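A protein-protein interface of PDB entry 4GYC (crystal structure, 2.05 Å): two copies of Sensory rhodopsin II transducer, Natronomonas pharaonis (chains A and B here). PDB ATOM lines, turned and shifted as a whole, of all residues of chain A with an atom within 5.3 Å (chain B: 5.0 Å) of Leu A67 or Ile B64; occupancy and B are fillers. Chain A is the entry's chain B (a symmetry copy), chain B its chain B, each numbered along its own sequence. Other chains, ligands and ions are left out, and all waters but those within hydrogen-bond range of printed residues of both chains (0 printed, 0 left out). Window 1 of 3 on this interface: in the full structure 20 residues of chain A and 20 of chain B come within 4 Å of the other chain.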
ATOM      1  N   THR A  33       8.633 -14.634  12.207  1.00  0.00           N
ATOM      2  CA  THR A  33       9.735 -13.730  11.923  1.00  0.00           C
ATOM      3  C   THR A  33       9.837 -12.587  12.945  1.00  0.00           C
ATOM      4  O   THR A  33      10.935 -12.220  13.375  1.00  0.00           O
ATOM      5  CB  THR A  33       9.616 -13.167  10.494  1.00  0.00           C
ATOM      6  OG1 THR A  33       9.610 -14.263   9.562  1.00  0.00           O
ATOM      7  CG2 THR A  33      10.792 -12.251  10.183  1.00  0.00           C
ATOM      8  N   PHE A  36      11.078 -14.114  16.189  1.00  0.00           N
ATOM      9  CA  PHE A  36      12.518 -14.279  16.096  1.00  0.00           C
ATOM     10  C   PHE A  36      13.248 -12.926  16.185  1.00  0.00           C
ATOM     11  O   PHE A  36      14.277 -12.813  16.851  1.00  0.00           O
ATOM     12  CB  PHE A  36      12.908 -15.020  14.817  1.00  0.00           C
ATOM     13  CG  PHE A  36      14.359 -15.386  14.767  1.00  0.00           C
ATOM     14  CD1 PHE A  36      14.794 -16.598  15.275  1.00  0.00           C
ATOM     15  CD2 PHE A  36      15.296 -14.500  14.259  1.00  0.00           C
ATOM     16  CE1 PHE A  36      16.136 -16.929  15.257  1.00  0.00           C
ATOM     17  CE2 PHE A  36      16.646 -14.825  14.238  1.00  0.00           C
ATOM     18  CZ  PHE A  36      17.064 -16.046  14.737  1.00  0.00           C
ATOM     19  N   GLY A  37      12.710 -11.904  15.523  1.00  0.00           N
ATOM     20  CA  GLY A  37      13.278 -10.568  15.603  1.00  0.00           C
ATOM     21  C   GLY A  37      13.333 -10.036  17.034  1.00  0.00           C
ATOM     22  O   GLY A  37      14.329  -9.435  17.454  1.00  0.00           O
ATOM     23  N   ALA A  40      16.156 -11.780  18.912  1.00  0.00           N
ATOM     24  CA  ALA A  40      17.426 -11.197  18.507  1.00  0.00           C
ATOM     25  C   ALA A  40      17.600  -9.795  19.078  1.00  0.00           C
ATOM     26  O   ALA A  40      18.701  -9.399  19.460  1.00  0.00           O
ATOM     27  CB  ALA A  40      17.519 -11.157  16.995  1.00  0.00           C
ATOM     28  N   TYR A  41      16.514  -9.030  19.102  1.00  0.00           N
ATOM     29  CA  TYR A  41      16.572  -7.672  19.613  1.00  0.00           C
ATOM     30  C   TYR A  41      16.902  -7.689  21.106  1.00  0.00           C
ATOM     31  O   TYR A  41      17.619  -6.829  21.599  1.00  0.00           O
ATOM     32  CB  TYR A  41      15.248  -6.940  19.376  1.00  0.00           C
ATOM     33  CG  TYR A  41      15.160  -5.621  20.110  1.00  0.00           C
ATOM     34  CD1 TYR A  41      15.869  -4.509  19.671  1.00  0.00           C
ATOM     35  CD2 TYR A  41      14.381  -5.490  21.254  1.00  0.00           C
ATOM     36  CE1 TYR A  41      15.802  -3.302  20.345  1.00  0.00           C
ATOM     37  CE2 TYR A  41      14.306  -4.285  21.938  1.00  0.00           C
ATOM     38  CZ  TYR A  41      15.017  -3.191  21.474  1.00  0.00           C
ATOM     39  OH  TYR A  41      14.951  -1.986  22.147  1.00  0.00           O
ATOM     40  N   VAL A  44      20.636  -8.111  21.623  1.00  0.00           N
ATOM     41  CA  VAL A  44      21.330  -6.857  21.313  1.00  0.00           C
ATOM     42  C   VAL A  44      21.237  -5.842  22.454  1.00  0.00           C
ATOM     43  O   VAL A  44      22.232  -5.204  22.811  1.00  0.00           O
ATOM     44  CB  VAL A  44      20.794  -6.214  20.015  1.00  0.00           C
ATOM     45  CG1 VAL A  44      21.297  -4.782  19.882  1.00  0.00           C
ATOM     46  CG2 VAL A  44      21.193  -7.044  18.815  1.00  0.00           C
ATOM     47  N   SER A  62      25.191 -12.427  15.159  1.00  0.00           N
ATOM     48  CA  SER A  62      24.334 -13.590  15.360  1.00  0.00           C
ATOM     49  C   SER A  62      22.915 -13.279  14.877  1.00  0.00           C
ATOM     50  O   SER A  62      22.278 -14.111  14.230  1.00  0.00           O
ATOM     51  CB  SER A  62      24.351 -13.970  16.847  1.00  0.00           C
ATOM     52  OG  SER A  62      23.334 -14.878  17.201  1.00  0.00           O
ATOM     53  N   ALA A  63      22.420 -12.079  15.167  1.00  0.00           N
ATOM     54  CA  ALA A  63      21.057 -11.717  14.760  1.00  0.00           C
ATOM     55  C   ALA A  63      20.916 -11.676  13.236  1.00  0.00           C
ATOM     56  O   ALA A  63      19.917 -12.130  12.676  1.00  0.00           O
ATOM     57  CB  ALA A  63      20.662 -10.390  15.358  1.00  0.00           C
ATOM     58  N   ILE A  64      21.930 -11.133  12.575  1.00  0.00           N
ATOM     59  CA  ILE A  64      21.923 -10.988  11.132  1.00  0.00           C
ATOM     60  C   ILE A  64      21.989 -12.349  10.426  1.00  0.00           C
ATOM     61  O   ILE A  64      21.177 -12.642   9.542  1.00  0.00           O
ATOM     62  CB  ILE A  64      23.074 -10.089  10.671  1.00  0.00           C
ATOM     63  CG1 ILE A  64      22.809  -8.634  11.071  1.00  0.00           C
ATOM     64  CG2 ILE A  64      23.261 -10.174   9.153  1.00  0.00           C
ATOM     65  CD1 ILE A  64      24.052  -7.762  10.980  1.00  0.00           C
ATOM     66  N   LEU A  65      22.946 -13.179  10.819  1.00  0.00           N
ATOM     67  CA  LEU A  65      23.041 -14.524  10.254  1.00  0.00           C
ATOM     68  C   LEU A  65      21.767 -15.325  10.512  1.00  0.00           C
ATOM     69  O   LEU A  65      21.258 -16.012   9.615  1.00  0.00           O
ATOM     70  CB  LEU A  65      24.242 -15.280  10.828  1.00  0.00           C
ATOM     71  CG  LEU A  65      25.608 -14.760  10.381  1.00  0.00           C
ATOM     72  CD1 LEU A  65      26.742 -15.396  11.206  1.00  0.00           C
ATOM     73  CD2 LEU A  65      25.787 -14.994   8.878  1.00  0.00           C
ATOM     74  N   GLY A  66      21.267 -15.241  11.743  1.00  0.00           N
ATOM     75  CA  GLY A  66      20.052 -15.935  12.131  1.00  0.00           C
ATOM     76  C   GLY A  66      18.846 -15.518  11.305  1.00  0.00           C
ATOM     77  O   GLY A  66      18.035 -16.351  10.904  1.00  0.00           O
ATOM     78  N   LEU A  67      18.730 -14.220  11.044  1.00  0.00           N
ATOM     79  CA  LEU A  67      17.629 -13.709  10.242  1.00  0.00           C
ATOM     80  C   LEU A  67      17.761 -14.120   8.775  1.00  0.00           C
ATOM     81  O   LEU A  67      16.766 -14.389   8.114  1.00  0.00           O
ATOM     82  CB  LEU A  67      17.507 -12.188  10.391  1.00  0.00           C
ATOM     83  CG  LEU A  67      16.756 -11.758  11.658  1.00  0.00           C
ATOM     84  CD1 LEU A  67      16.998 -10.277  12.005  1.00  0.00           C
ATOM     85  CD2 LEU A  67      15.264 -12.039  11.519  1.00  0.00           C
ATOM     86  N   ILE A  68      18.991 -14.173   8.267  1.00  0.00           N
ATOM     87  CA  ILE A  68      19.222 -14.680   6.913  1.00  0.00           C
ATOM     88  C   ILE A  68      18.824 -16.160   6.823  1.00  0.00           C
ATOM     89  O   ILE A  68      18.156 -16.585   5.883  1.00  0.00           O
ATOM     90  CB  ILE A  68      20.704 -14.529   6.494  1.00  0.00           C
ATOM     91  CG1 ILE A  68      21.061 -13.053   6.287  1.00  0.00           C
ATOM     92  CG2 ILE A  68      20.975 -15.315   5.194  1.00  0.00           C
ATOM     93  CD1 ILE A  68      22.585 -12.808   6.141  1.00  0.00           C
ATOM     94  N   ILE A  69      19.248 -16.944   7.808  1.00  0.00           N
ATOM     95  CA  ILE A  69      18.891 -18.359   7.849  1.00  0.00           C
ATOM     96  C   ILE A  69      17.367 -18.521   7.938  1.00  0.00           C
ATOM     97  O   ILE A  69      16.783 -19.354   7.244  1.00  0.00           O
ATOM     98  CB  ILE A  69      19.611 -19.081   9.016  1.00  0.00           C
ATOM     99  CG1 ILE A  69      21.115 -19.185   8.709  1.00  0.00           C
ATOM    100  CG2 ILE A  69      19.026 -20.484   9.237  1.00  0.00           C
ATOM    101  CD1 ILE A  69      21.993 -19.522   9.968  1.00  0.00           C
ATOM    102  N   LEU A  70      16.738 -17.706   8.788  1.00  0.00           N
ATOM    103  CA  LEU A  70      15.294 -17.703   8.948  1.00  0.00           C
ATOM    104  C   LEU A  70      14.589 -17.440   7.615  1.00  0.00           C
ATOM    105  O   LEU A  70      13.584 -18.070   7.311  1.00  0.00           O
ATOM    106  CB  LEU A  70      14.844 -16.680   9.994  1.00  0.00           C
ATOM    107  CG  LEU A  70      13.361 -16.809  10.393  1.00  0.00           C
ATOM    108  CD1 LEU A  70      13.148 -18.019  11.277  1.00  0.00           C
ATOM    109  CD2 LEU A  70      12.845 -15.584  11.109  1.00  0.00           C
ATOM    110  N   LEU A  71      15.111 -16.519   6.813  1.00  0.00           N
ATOM    111  CA  LEU A  71      14.546 -16.320   5.479  1.00  0.00           C
ATOM    112  C   LEU A  71      14.566 -17.607   4.665  1.00  0.00           C
ATOM    113  O   LEU A  71      13.582 -17.956   4.012  1.00  0.00           O
ATOM    114  CB  LEU A  71      15.295 -15.224   4.702  1.00  0.00           C
ATOM    115  CG  LEU A  71      14.960 -15.361   3.203  1.00  0.00           C
ATOM    116  CD1 LEU A  71      13.554 -14.824   2.877  1.00  0.00           C
ATOM    117  CD2 LEU A  71      16.009 -14.715   2.287  1.00  0.00           C
ATOM    118  N   ALA B  60      22.401  -2.218  14.867  1.00  0.00           N
ATOM    119  CA  ALA B  60      21.909  -3.583  14.937  1.00  0.00           C
ATOM    120  C   ALA B  60      20.390  -3.597  14.907  1.00  0.00           C
ATOM    121  O   ALA B  60      19.774  -4.478  14.304  1.00  0.00           O
ATOM    122  CB  ALA B  60      22.443  -4.276  16.218  1.00  0.00           C
ATOM    123  N   VAL B  61      19.777  -2.624  15.572  1.00  0.00           N
ATOM    124  CA  VAL B  61      18.323  -2.525  15.569  1.00  0.00           C
ATOM    125  C   VAL B  61      17.840  -2.237  14.154  1.00  0.00           C
ATOM    126  O   VAL B  61      16.846  -2.798  13.698  1.00  0.00           O
ATOM    127  CB  VAL B  61      17.822  -1.443  16.546  1.00  0.00           C
ATOM    128  CG1 VAL B  61      16.340  -1.153  16.313  1.00  0.00           C
ATOM    129  CG2 VAL B  61      18.070  -1.892  18.004  1.00  0.00           C
ATOM    130  N   SER B  62      18.556  -1.356  13.467  1.00  0.00           N
ATOM    131  CA  SER B  62      18.289  -1.050  12.066  1.00  0.00           C
ATOM    132  C   SER B  62      18.460  -2.312  11.217  1.00  0.00           C
ATOM    133  O   SER B  62      17.655  -2.580  10.325  1.00  0.00           O
ATOM    134  CB  SER B  62      19.238   0.067  11.611  1.00  0.00           C
ATOM    135  OG  SER B  62      19.276   0.229  10.212  1.00  0.00           O
ATOM    136  N   ALA B  63      19.491  -3.104  11.500  1.00  0.00           N
ATOM    137  CA  ALA B  63      19.737  -4.318  10.713  1.00  0.00           C
ATOM    138  C   ALA B  63      18.601  -5.333  10.874  1.00  0.00           C
ATOM    139  O   ALA B  63      18.171  -5.968   9.910  1.00  0.00           O
ATOM    140  CB  ALA B  63      21.054  -4.942  11.100  1.00  0.00           C
ATOM    141  N   ILE B  64      18.118  -5.471  12.102  1.00  0.00           N
ATOM    142  CA  ILE B  64      17.068  -6.421  12.418  1.00  0.00           C
ATOM    143  C   ILE B  64      15.734  -6.028  11.770  1.00  0.00           C
ATOM    144  O   ILE B  64      15.092  -6.844  11.101  1.00  0.00           O
ATOM    145  CB  ILE B  64      16.906  -6.567  13.934  1.00  0.00           C
ATOM    146  CG1 ILE B  64      18.105  -7.309  14.532  1.00  0.00           C
ATOM    147  CG2 ILE B  64      15.617  -7.321  14.276  1.00  0.00           C
ATOM    148  CD1 ILE B  64      18.194  -7.166  16.043  1.00  0.00           C
ATOM    149  N   LEU B  65      15.324  -4.780  11.960  1.00  0.00           N
ATOM    150  CA  LEU B  65      14.101  -4.295  11.322  1.00  0.00           C
ATOM    151  C   LEU B  65      14.193  -4.396   9.801  1.00  0.00           C
ATOM    152  O   LEU B  65      13.238  -4.824   9.137  1.00  0.00           O
ATOM    153  CB  LEU B  65      13.810  -2.846  11.719  1.00  0.00           C
ATOM    154  CG  LEU B  65      13.388  -2.644  13.174  1.00  0.00           C
ATOM    155  CD1 LEU B  65      13.379  -1.151  13.550  1.00  0.00           C
ATOM    156  CD2 LEU B  65      12.031  -3.309  13.418  1.00  0.00           C
ATOM    157  N   GLY B  66      15.337  -3.987   9.260  1.00  0.00           N
ATOM    158  CA  GLY B  66      15.575  -4.038   7.828  1.00  0.00           C
ATOM    159  C   GLY B  66      15.481  -5.448   7.265  1.00  0.00           C
ATOM    160  O   GLY B  66      14.914  -5.665   6.196  1.00  0.00           O
ATOM    161  N   LEU B  67      16.034  -6.413   7.993  1.00  0.00           N
ATOM    162  CA  LEU B  67      15.983  -7.802   7.564  1.00  0.00           C
ATOM    163  C   LEU B  67      14.566  -8.370   7.661  1.00  0.00           C
ATOM    164  O   LEU B  67      14.161  -9.169   6.827  1.00  0.00           O
ATOM    165  CB  LEU B  67      16.985  -8.652   8.355  1.00  0.00           C
ATOM    166  CG  LEU B  67      18.419  -8.561   7.817  1.00  0.00           C
ATOM    167  CD1 LEU B  67      19.457  -9.066   8.837  1.00  0.00           C
ATOM    168  CD2 LEU B  67      18.547  -9.319   6.501  1.00  0.00           C
ATOM    169  N   ILE B  68      13.813  -7.955   8.676  1.00  0.00           N
ATOM    170  CA  ILE B  68      12.405  -8.345   8.775  1.00  0.00           C
ATOM    171  C   ILE B  68      11.610  -7.774   7.592  1.00  0.00           C
ATOM    172  O   ILE B  68      10.811  -8.468   6.965  1.00  0.00           O
ATOM    173  CB  ILE B  68      11.767  -7.851  10.095  1.00  0.00           C
ATOM    174  CG1 ILE B  68      12.337  -8.620  11.292  1.00  0.00           C
ATOM    175  CG2 ILE B  68      10.235  -8.028  10.049  1.00  0.00           C
ATOM    176  CD1 ILE B  68      11.957  -7.994  12.659  1.00  0.00           C
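Of the printed residues of chain B, Tyr A41 touches Val B61 and Ile B64. Of the printed residues of chain B, Ile A64 touches Leu B67. Printed residues of chain B within 4 Å of Leu A67: Ile B64 (3.9 Å) and Leu B67 (3.995 Å). Ile B64 touches just these residues of chain A: Tyr A41 (3.95 Å) and Leu A67 (3.9 Å). The nearest printed residue of chain B that does not touch Leu A67 is Ile B68 (4.5 Å). The nearest residue of chain A that does not touch Ile B64 is Gly A37 (4.03 Å). The nearest printed residue of chain B that does not touch Val A44 is Ile B64 (4.1 Å).
Hydrophobic or aromatic side chains of chain B that line the printed part of chain A: Ala B60, Val B61, Ile B64 and Leu B67. Of the 16 printed residues of chain A, 4 touch a printed residue of chain B. Printed residues of chain A that touch a printed residue of chain B: Tyr A41, Val A44, Ile A64 and Leu A67. Hydrophobic or aromatic side chains of chain A within 4 Å of the printed part of chain B: Tyr A41, Val A44, Ile A64 and Leu A67. Among the printed residues, no Asp or Glu carboxylate lies within 4 Å of a Lys or Arg side-chain nitrogen of the other chain.
Among the printed residues, merely in contact across the chains: Tyr A41 with Val B61, Val A44 with Ala B60, Ile A64 with Leu B67, Leu A67 with Ile B64, Tyr A41 with Ile B64 and Leu A67 with Leu B67.
Ile A64 touches Leu B67, and with the chains exchanged Leu A67 touches Ile B64. Leu A67 touches its own counterpart, Leu B67. 7 positions are printed for both chains.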
